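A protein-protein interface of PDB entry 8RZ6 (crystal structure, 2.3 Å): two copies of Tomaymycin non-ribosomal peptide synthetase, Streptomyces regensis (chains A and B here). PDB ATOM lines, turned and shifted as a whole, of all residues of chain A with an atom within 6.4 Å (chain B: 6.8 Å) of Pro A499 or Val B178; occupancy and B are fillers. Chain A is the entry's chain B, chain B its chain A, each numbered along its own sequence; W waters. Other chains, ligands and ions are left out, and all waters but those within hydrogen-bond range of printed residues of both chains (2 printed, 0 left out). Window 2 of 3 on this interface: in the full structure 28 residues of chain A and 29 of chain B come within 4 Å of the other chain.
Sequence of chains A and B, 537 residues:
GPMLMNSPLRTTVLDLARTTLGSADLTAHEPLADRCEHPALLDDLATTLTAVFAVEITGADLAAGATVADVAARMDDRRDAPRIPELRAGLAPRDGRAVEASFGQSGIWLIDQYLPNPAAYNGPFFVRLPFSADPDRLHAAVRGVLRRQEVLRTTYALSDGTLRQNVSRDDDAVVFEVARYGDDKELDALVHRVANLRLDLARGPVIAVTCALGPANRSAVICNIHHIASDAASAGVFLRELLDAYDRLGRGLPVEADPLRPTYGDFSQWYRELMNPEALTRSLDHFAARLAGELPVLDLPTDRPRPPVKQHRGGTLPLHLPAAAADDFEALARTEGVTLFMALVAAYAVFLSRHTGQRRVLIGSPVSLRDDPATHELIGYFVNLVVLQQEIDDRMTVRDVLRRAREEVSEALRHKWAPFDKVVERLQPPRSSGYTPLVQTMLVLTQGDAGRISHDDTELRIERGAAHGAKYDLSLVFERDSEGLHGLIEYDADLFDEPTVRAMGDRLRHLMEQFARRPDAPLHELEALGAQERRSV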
ATOM      1  N   ASP A 303     -22.377   0.230  25.066  1.00  0.00           N
ATOM      2  CA  ASP A 303     -22.678   1.622  24.762  1.00  0.00           C
ATOM      3  C   ASP A 303     -23.205   2.342  25.985  1.00  0.00           C
ATOM      4  O   ASP A 303     -23.078   3.557  26.090  1.00  0.00           O
ATOM      5  CB  ASP A 303     -23.653   1.659  23.588  1.00  0.00           C
ATOM      6  CG  ASP A 303     -23.047   1.040  22.325  1.00  0.00           C
ATOM      7  OD1 ASP A 303     -22.185   1.680  21.729  1.00  0.00           O
ATOM      8  OD2 ASP A 303     -23.418  -0.077  21.931  1.00  0.00           O
ATOM      9  N   ARG A 304     -23.737   1.613  26.949  1.00  0.00           N
ATOM     10  CA  ARG A 304     -24.290   2.220  28.141  1.00  0.00           C
ATOM     11  C   ARG A 304     -23.832   1.380  29.314  1.00  0.00           C
ATOM     12  O   ARG A 304     -23.729   0.158  29.186  1.00  0.00           O
ATOM     13  CB  ARG A 304     -25.831   2.257  28.118  1.00  0.00           C
ATOM     14  CG  ARG A 304     -26.437   3.233  27.107  1.00  0.00           C
ATOM     15  CD  ARG A 304     -27.970   2.984  26.981  1.00  0.00           C
ATOM     16  NE  ARG A 304     -28.268   1.865  26.089  1.00  0.00           N
ATOM     17  CZ  ARG A 304     -28.123   1.916  24.768  1.00  0.00           C
ATOM     18  NH1 ARG A 304     -27.701   3.017  24.153  1.00  0.00           N
ATOM     19  NH2 ARG A 304     -28.396   0.836  24.046  1.00  0.00           N
ATOM     20  N   LEU A 317     -30.120 -10.015  16.369  1.00  0.00           N
ATOM     21  CA  LEU A 317     -29.367  -9.661  15.185  1.00  0.00           C
ATOM     22  C   LEU A 317     -28.914 -10.938  14.494  1.00  0.00           C
ATOM     23  O   LEU A 317     -28.237 -11.771  15.111  1.00  0.00           O
ATOM     24  CB  LEU A 317     -28.187  -8.757  15.521  1.00  0.00           C
ATOM     25  CG  LEU A 317     -27.847  -7.840  14.361  1.00  0.00           C
ATOM     26  CD1 LEU A 317     -29.000  -6.921  13.921  1.00  0.00           C
ATOM     27  CD2 LEU A 317     -26.649  -7.039  14.757  1.00  0.00           C
ATOM     28  N   TYR A 491     -29.459  -9.955  22.375  1.00  0.00           N
ATOM     29  CA  TYR A 491     -28.633  -9.026  23.131  1.00  0.00           C
ATOM     30  C   TYR A 491     -29.494  -8.125  23.994  1.00  0.00           C
ATOM     31  O   TYR A 491     -30.677  -7.934  23.732  1.00  0.00           O
ATOM     32  CB  TYR A 491     -27.745  -8.160  22.225  1.00  0.00           C
ATOM     33  CG  TYR A 491     -28.454  -7.094  21.400  1.00  0.00           C
ATOM     34  CD1 TYR A 491     -28.935  -7.382  20.123  1.00  0.00           C
ATOM     35  CD2 TYR A 491     -28.622  -5.800  21.886  1.00  0.00           C
ATOM     36  CE1 TYR A 491     -29.580  -6.428  19.363  1.00  0.00           C
ATOM     37  CE2 TYR A 491     -29.235  -4.827  21.119  1.00  0.00           C
ATOM     38  CZ  TYR A 491     -29.699  -5.154  19.852  1.00  0.00           C
ATOM     39  OH  TYR A 491     -30.302  -4.197  19.081  1.00  0.00           O
ATOM     40  N   PHE A 496     -26.383  -2.333  24.764  1.00  0.00           N
ATOM     41  CA  PHE A 496     -25.875  -2.241  23.410  1.00  0.00           C
ATOM     42  C   PHE A 496     -26.855  -1.530  22.469  1.00  0.00           C
ATOM     43  O   PHE A 496     -28.075  -1.779  22.492  1.00  0.00           O
ATOM     44  CB  PHE A 496     -25.592  -3.628  22.862  1.00  0.00           C
ATOM     45  CG  PHE A 496     -24.613  -4.465  23.660  1.00  0.00           C
ATOM     46  CD1 PHE A 496     -23.259  -4.112  23.733  1.00  0.00           C
ATOM     47  CD2 PHE A 496     -25.043  -5.682  24.257  1.00  0.00           C
ATOM     48  CE1 PHE A 496     -22.357  -4.929  24.398  1.00  0.00           C
ATOM     49  CE2 PHE A 496     -24.152  -6.506  24.935  1.00  0.00           C
ATOM     50  CZ  PHE A 496     -22.797  -6.140  24.988  1.00  0.00           C
ATOM     51  N   ASP A 497     -26.295  -0.672  21.639  1.00  0.00           N
ATOM     52  CA  ASP A 497     -26.935  -0.241  20.414  1.00  0.00           C
ATOM     53  C   ASP A 497     -26.670  -1.253  19.304  1.00  0.00           C
ATOM     54  O   ASP A 497     -25.631  -1.926  19.279  1.00  0.00           O
ATOM     55  CB  ASP A 497     -26.420   1.130  19.961  1.00  0.00           C
ATOM     56  CG  ASP A 497     -26.643   2.211  20.981  1.00  0.00           C
ATOM     57  OD1 ASP A 497     -27.691   2.172  21.660  1.00  0.00           O
ATOM     58  OD2 ASP A 497     -25.755   3.080  21.099  1.00  0.00           O
ATOM     59  N   GLU A 498     -27.587  -1.302  18.349  1.00  0.00           N
ATOM     60  CA  GLU A 498     -27.538  -2.362  17.347  1.00  0.00           C
ATOM     61  C   GLU A 498     -26.257  -2.365  16.530  1.00  0.00           C
ATOM     62  O   GLU A 498     -25.796  -3.467  16.181  1.00  0.00           O
ATOM     63  CB  GLU A 498     -28.761  -2.253  16.430  1.00  0.00           C
ATOM     64  CG  GLU A 498     -28.819  -3.308  15.350  1.00  0.00           C
ATOM     65  CD  GLU A 498     -30.054  -3.240  14.494  1.00  0.00           C
ATOM     66  OE1 GLU A 498     -31.137  -2.871  15.003  1.00  0.00           O
ATOM     67  OE2 GLU A 498     -29.925  -3.560  13.302  1.00  0.00           O
ATOM     68  N   PRO A 499     -25.684  -1.223  16.130  1.00  0.00           N
ATOM     69  CA  PRO A 499     -24.454  -1.260  15.314  1.00  0.00           C
ATOM     70  C   PRO A 499     -23.262  -1.827  16.068  1.00  0.00           C
ATOM     71  O   PRO A 499     -22.334  -2.371  15.455  1.00  0.00           O
ATOM     72  CB  PRO A 499     -24.233   0.219  14.941  1.00  0.00           C
ATOM     73  CG  PRO A 499     -25.586   0.818  15.033  1.00  0.00           C
ATOM     74  CD  PRO A 499     -26.263   0.132  16.182  1.00  0.00           C
ATOM     75  N   THR A 500     -23.241  -1.661  17.390  1.00  0.00           N
ATOM     76  CA  THR A 500     -22.247  -2.337  18.207  1.00  0.00           C
ATOM     77  C   THR A 500     -22.415  -3.845  18.077  1.00  0.00           C
ATOM     78  O   THR A 500     -21.440  -4.565  17.891  1.00  0.00           O
ATOM     79  CB  THR A 500     -22.381  -1.901  19.666  1.00  0.00           C
ATOM     80  OG1 THR A 500     -22.344  -0.469  19.764  1.00  0.00           O
ATOM     81  CG2 THR A 500     -21.268  -2.505  20.519  1.00  0.00           C
ATOM     82  N   VAL A 501     -23.657  -4.338  18.106  1.00  0.00           N
ATOM     83  CA  VAL A 501     -23.858  -5.773  18.045  1.00  0.00           C
ATOM     84  C   VAL A 501     -23.563  -6.284  16.649  1.00  0.00           C
ATOM     85  O   VAL A 501     -23.055  -7.397  16.484  1.00  0.00           O
ATOM     86  CB  VAL A 501     -25.266  -6.141  18.521  1.00  0.00           C
ATOM     87  CG1 VAL A 501     -25.462  -7.647  18.504  1.00  0.00           C
ATOM     88  CG2 VAL A 501     -25.494  -5.607  19.902  1.00  0.00           C
ATOM     89  N   ARG A 502     -23.854  -5.481  15.626  1.00  0.00           N
ATOM     90  CA  ARG A 502     -23.502  -5.854  14.258  1.00  0.00           C
ATOM     91  C   ARG A 502     -21.984  -5.967  14.086  1.00  0.00           C
ATOM     92  O   ARG A 502     -21.505  -6.868  13.400  1.00  0.00           O
ATOM     93  CB  ARG A 502     -24.112  -4.832  13.292  1.00  0.00           C
ATOM     94  CG  ARG A 502     -23.650  -4.888  11.832  1.00  0.00           C
ATOM     95  CD  ARG A 502     -23.521  -6.272  11.261  1.00  0.00           C
ATOM     96  NE  ARG A 502     -24.717  -7.072  11.417  1.00  0.00           N
ATOM     97  CZ  ARG A 502     -24.735  -8.399  11.467  1.00  0.00           C
ATOM     98  NH1 ARG A 502     -23.623  -9.117  11.373  1.00  0.00           N
ATOM     99  NH2 ARG A 502     -25.901  -9.024  11.617  1.00  0.00           N
ATOM    100  N   ALA A 503     -21.217  -5.085  14.723  1.00  0.00           N
ATOM    101  CA  ALA A 503     -19.763  -5.179  14.635  1.00  0.00           C
ATOM    102  C   ALA A 503     -19.228  -6.404  15.388  1.00  0.00           C
ATOM    103  O   ALA A 503     -18.282  -7.064  14.932  1.00  0.00           O
ATOM    104  CB  ALA A 503     -19.134  -3.885  15.159  1.00  0.00           C
ATOM    105  N   MET A 504     -19.825  -6.739  16.526  1.00  0.00           N
ATOM    106  CA  MET A 504     -19.472  -7.972  17.207  1.00  0.00           C
ATOM    107  C   MET A 504     -19.749  -9.215  16.366  1.00  0.00           C
ATOM    108  O   MET A 504     -18.892 -10.137  16.244  1.00  0.00           O
ATOM    109  CB  MET A 504     -20.224  -8.113  18.537  1.00  0.00           C
ATOM    110  CG  MET A 504     -19.668  -7.193  19.603  1.00  0.00           C
ATOM    111  SD  MET A 504     -20.509  -7.436  21.371  1.00  0.00           S
ATOM    112  CE  MET A 504     -20.166  -9.278  21.745  1.00  0.00           C
ATOM    113  N   PRO B 135     -27.209  10.350  15.886  1.00  0.00           N
ATOM    114  CA  PRO B 135     -27.665   9.769  17.174  1.00  0.00           C
ATOM    115  C   PRO B 135     -27.157  10.507  18.403  1.00  0.00           C
ATOM    116  O   PRO B 135     -27.901  10.656  19.386  1.00  0.00           O
ATOM    117  CB  PRO B 135     -27.122   8.330  17.134  1.00  0.00           C
ATOM    118  CG  PRO B 135     -26.860   8.039  15.697  1.00  0.00           C
ATOM    119  CD  PRO B 135     -26.522   9.355  15.023  1.00  0.00           C
ATOM    120  N   ASP B 136     -25.905  10.972  18.390  1.00  0.00           N
ATOM    121  CA  ASP B 136     -25.379  11.637  19.580  1.00  0.00           C
ATOM    122  C   ASP B 136     -26.058  12.973  19.792  1.00  0.00           C
ATOM    123  O   ASP B 136     -26.406  13.330  20.919  1.00  0.00           O
ATOM    124  CB  ASP B 136     -23.859  11.827  19.483  1.00  0.00           C
ATOM    125  CG  ASP B 136     -23.111  10.499  19.465  1.00  0.00           C
ATOM    126  OD1 ASP B 136     -23.497   9.577  20.229  1.00  0.00           O
ATOM    127  OD2 ASP B 136     -22.156  10.375  18.669  1.00  0.00           O
ATOM    128  N   PHE B 176     -32.855   4.714  26.406  1.00  0.00           N
ATOM    129  CA  PHE B 176     -32.384   5.112  25.088  1.00  0.00           C
ATOM    130  C   PHE B 176     -31.664   3.969  24.376  1.00  0.00           C
ATOM    131  O   PHE B 176     -31.057   3.081  24.995  1.00  0.00           O
ATOM    132  CB  PHE B 176     -31.451   6.351  25.223  1.00  0.00           C
ATOM    133  CG  PHE B 176     -31.111   7.016  23.914  1.00  0.00           C
ATOM    134  CD1 PHE B 176     -31.963   7.950  23.355  1.00  0.00           C
ATOM    135  CD2 PHE B 176     -29.941   6.723  23.254  1.00  0.00           C
ATOM    136  CE1 PHE B 176     -31.665   8.574  22.151  1.00  0.00           C
ATOM    137  CE2 PHE B 176     -29.635   7.336  22.025  1.00  0.00           C
ATOM    138  CZ  PHE B 176     -30.495   8.264  21.487  1.00  0.00           C
ATOM    139  N   GLU B 177     -31.730   4.018  23.045  1.00  0.00           N
ATOM    140  CA  GLU B 177     -30.982   3.077  22.215  1.00  0.00           C
ATOM    141  C   GLU B 177     -30.946   3.634  20.813  1.00  0.00           C
ATOM    142  O   GLU B 177     -31.802   4.429  20.436  1.00  0.00           O
ATOM    143  CB  GLU B 177     -31.585   1.653  22.199  1.00  0.00           C
ATOM    144  CG  GLU B 177     -32.979   1.520  21.745  1.00  0.00           C
ATOM    145  CD  GLU B 177     -33.440   0.067  21.502  1.00  0.00           C
ATOM    146  OE1 GLU B 177     -32.733  -0.710  20.840  1.00  0.00           O
ATOM    147  OE2 GLU B 177     -34.557  -0.280  21.955  1.00  0.00           O
ATOM    148  N   VAL B 178     -29.950   3.185  20.045  1.00  0.00           N
ATOM    149  CA  VAL B 178     -29.846   3.413  18.607  1.00  0.00           C
ATOM    150  C   VAL B 178     -30.028   2.067  17.919  1.00  0.00           C
ATOM    151  O   VAL B 178     -29.304   1.106  18.230  1.00  0.00           O
ATOM    152  CB  VAL B 178     -28.474   4.025  18.238  1.00  0.00           C
ATOM    153  CG1 VAL B 178     -28.405   4.365  16.785  1.00  0.00           C
ATOM    154  CG2 VAL B 178     -28.174   5.261  19.045  1.00  0.00           C
ATOM    155  N   ALA B 179     -30.964   1.989  16.958  1.00  0.00           N
ATOM    156  CA  ALA B 179     -31.186   0.748  16.214  1.00  0.00           C
ATOM    157  C   ALA B 179     -31.455   1.055  14.751  1.00  0.00           C
ATOM    158  O   ALA B 179     -31.547   2.211  14.355  1.00  0.00           O
ATOM    159  CB  ALA B 179     -32.331  -0.070  16.815  1.00  0.00           C
ATOM    160  N   ARG B 180     -31.520   0.000  13.929  1.00  0.00           N
ATOM    161  CA  ARG B 180     -31.675   0.132  12.486  1.00  0.00           C
ATOM    162  C   ARG B 180     -32.958  -0.545  11.999  1.00  0.00           C
ATOM    163  O   ARG B 180     -33.526  -1.402  12.662  1.00  0.00           O
ATOM    164  CB  ARG B 180     -30.476  -0.451  11.722  1.00  0.00           C
ATOM    165  CG  ARG B 180     -29.126   0.194  12.042  1.00  0.00           C
ATOM    166  CD  ARG B 180     -28.102   0.011  10.891  1.00  0.00           C
ATOM    167  NE  ARG B 180     -27.357   1.244  10.662  1.00  0.00           N
ATOM    168  CZ  ARG B 180     -27.756   2.240   9.877  1.00  0.00           C
ATOM    169  NH1 ARG B 180     -28.856   2.152   9.145  1.00  0.00           N
ATOM    170  NH2 ARG B 180     -27.028   3.352   9.828  1.00  0.00           N
ATOM    171  N   LEU B 190     -39.109  -2.190  16.044  1.00  0.00           N
ATOM    172  CA  LEU B 190     -38.488  -1.271  17.019  1.00  0.00           C
ATOM    173  C   LEU B 190     -39.533  -0.540  17.853  1.00  0.00           C
ATOM    174  O   LEU B 190     -39.358  -0.358  19.063  1.00  0.00           O
ATOM    175  CB  LEU B 190     -37.577  -0.254  16.330  1.00  0.00           C
ATOM    176  CG  LEU B 190     -36.445  -0.866  15.512  1.00  0.00           C
ATOM    177  CD1 LEU B 190     -35.764   0.239  14.750  1.00  0.00           C
ATOM    178  CD2 LEU B 190     -35.398  -1.609  16.405  1.00  0.00           C
ATOM    179  N   ARG B 193     -40.761  -2.819  20.660  1.00  0.00           N
ATOM    180  CA  ARG B 193     -39.865  -2.897  21.804  1.00  0.00           C
ATOM    181  C   ARG B 193     -40.051  -1.680  22.706  1.00  0.00           C
ATOM    182  O   ARG B 193     -40.216  -1.809  23.922  1.00  0.00           O
ATOM    183  CB  ARG B 193     -38.412  -3.038  21.328  1.00  0.00           C
ATOM    184  CG  ARG B 193     -37.367  -2.890  22.430  1.00  0.00           C
ATOM    185  CD  ARG B 193     -36.093  -3.649  22.074  1.00  0.00           C
ATOM    186  NE  ARG B 193     -35.265  -2.970  21.089  1.00  0.00           N
ATOM    187  CZ  ARG B 193     -34.786  -3.514  19.977  1.00  0.00           C
ATOM    188  NH1 ARG B 193     -35.161  -4.708  19.575  1.00  0.00           N
ATOM    189  NH2 ARG B 193     -33.891  -2.838  19.251  1.00  0.00           N
ATOM    190  N   VAL B 209     -36.747   6.730  24.595  1.00  0.00           N
ATOM    191  CA  VAL B 209     -36.575   7.217  23.233  1.00  0.00           C
ATOM    192  C   VAL B 209     -35.626   6.298  22.495  1.00  0.00           C
ATOM    193  O   VAL B 209     -34.530   6.004  22.980  1.00  0.00           O
ATOM    194  CB  VAL B 209     -36.024   8.652  23.166  1.00  0.00           C
ATOM    195  CG1 VAL B 209     -35.752   9.038  21.728  1.00  0.00           C
ATOM    196  CG2 VAL B 209     -36.972   9.647  23.823  1.00  0.00           C
ATOM    197  N   THR B 210     -35.998   5.935  21.282  1.00  0.00           N
ATOM    198  CA  THR B 210     -35.104   5.255  20.364  1.00  0.00           C
ATOM    199  C   THR B 210     -34.848   6.138  19.157  1.00  0.00           C
ATOM    200  O   THR B 210     -35.793   6.675  18.564  1.00  0.00           O
ATOM    201  CB  THR B 210     -35.680   3.926  19.896  1.00  0.00           C
ATOM    202  OG1 THR B 210     -35.691   3.011  20.990  1.00  0.00           O
ATOM    203  CG2 THR B 210     -34.838   3.370  18.756  1.00  0.00           C
ATOM    204  N   CYS B 211     -33.575   6.286  18.807  1.00  0.00           N
ATOM    205  CA  CYS B 211     -33.151   6.889  17.544  1.00  0.00           C
ATOM    206  C   CYS B 211     -33.015   5.768  16.521  1.00  0.00           C
ATOM    207  O   CYS B 211     -32.055   4.977  16.563  1.00  0.00           O
ATOM    208  CB  CYS B 211     -31.831   7.657  17.733  1.00  0.00           C
ATOM    209  SG  CYS B 211     -31.132   8.277  16.156  1.00  0.00           S
ATOM    210  N   ALA B 212     -33.961   5.695  15.588  1.00  0.00           N
ATOM    211  CA  ALA B 212     -33.992   4.598  14.621  1.00  0.00           C
ATOM    212  C   ALA B 212     -33.427   5.078  13.295  1.00  0.00           C
ATOM    213  O   ALA B 212     -33.974   6.005  12.681  1.00  0.00           O
ATOM    214  CB  ALA B 212     -35.411   4.045  14.439  1.00  0.00           C
ATOM    215  N   LEU B 213     -32.369   4.425  12.843  1.00  0.00           N
ATOM    216  CA  LEU B 213     -31.693   4.788  11.603  1.00  0.00           C
ATOM    217  C   LEU B 213     -32.243   3.941  10.468  1.00  0.00           C
ATOM    218  O   LEU B 213     -32.189   2.696  10.528  1.00  0.00           O
ATOM    219  CB  LEU B 213     -30.179   4.608  11.733  1.00  0.00           C
ATOM    220  CG  LEU B 213     -29.631   5.404  12.950  1.00  0.00           C
ATOM    221  CD1 LEU B 213     -28.127   5.230  13.195  1.00  0.00           C
ATOM    222  CD2 LEU B 213     -29.976   6.885  12.842  1.00  0.00           C
HETATM  223  O   HOH W   1     -30.130  -1.629  20.374  1.00  0.00           O
HETATM  224  O   HOH W   2     -32.273  -4.156  17.184  1.00  0.00           O
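Water W2 lies within hydrogen-bond range of the side-chain hydroxyl of Tyr A491, the side-chain carboxylate of Glu A498 and the guanidinium group of Arg B193.
Water W1 lies within hydrogen-bond range of OE1 of Glu B177 (2.8 Å), OH of Tyr A491 (2.9 Å), O of Phe A496 (3.0 Å) and N of Glu A498 (3.3 Å).
Glu B177 touches Arg A304.
OH of Tyr A491 touches NH2 of Arg B193 (3.8 Å).
Glu B177 touches Asp A497 (CA to OD1, 3.5 Å).
Glu A498 touches Ala B179 (OE1 to CB, 3.5 Å).
Pro A499 touches Val B178.
Hydrophobic or aromatic side chains of chain A within 4 Å of the printed part of chain B: Tyr A491 and Pro A499.
Hydrophobic or aromatic side chains of chain B that line the printed part of chain A: Val B178 and Ala B179.
Among the printed residues, 9 pairs touch across the chains.
Among the printed residues, no Asp or Glu carboxylate lies within 4 Å of a Lys or Arg side-chain nitrogen of the other chain.
The backbone NH (N) of Arg B180 lies within hydrogen-bond range of the side-chain carboxylate (OE1) of Glu A498 (3.1 Å).
O of Val B178 lies within hydrogen-bond range of N of Glu A498 (3.0 Å).
The backbone NH (N) of Val B178 lies within hydrogen-bond range of the side-chain carboxylate (OD1) of Asp A497 (3.0 Å).
The guanidinium group of Arg A304 lies close to the backbone carbonyl oxygen of Phe B176 (3.2 Å).
No position is printed for both chains.
N of Asp A497 lies within hydrogen-bond range of OD2 of Asp A303 (3.0 Å).
The guanidinium group (NH2) of Arg A304 lies within hydrogen-bond range of the backbone carbonyl oxygen (O) of Phe A496 (3.1 Å).
The backbone NH (N) of Ala B179 is in hydrogen-bond range of the backbone carbonyl oxygen (O) of Cys B211, at 3.2 Å.
O of Ala B179 sits at hydrogen-bond distance from N of Leu B213 (2.8 Å).
O of Val B209 sits at hydrogen-bond distance from N of Glu B177 (3.4 Å).
N of Cys B211 is in hydrogen-bond range of O of Glu B177 (3.0 Å).
Pro A499 touches just one residue of chain B: Val B178 (3.8 Å).
Val B178 touches three residues of chain A.
Of the printed residues of chain A, Ala B179 touches Glu A498 (3.5 Å).
Printed residues of chain B within 4 Å of Asp A497: Glu B177 (3.5 Å) and Val B178 (3.0 Å).
Of the printed residues of chain B, Arg A304 touches Phe B176 (3.2 Å) and Glu B177 (3.8 Å).
Val A501 touches none of the printed residues of chain B.
Asp B136 touches none of the printed residues of chain A.
The nearest residue of chain A that does not touch Val B178 is Arg A304 (4.7 Å).
The nearest printed residue of chain B that does not touch Asp A497 is Phe B176 (4.8 Å).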
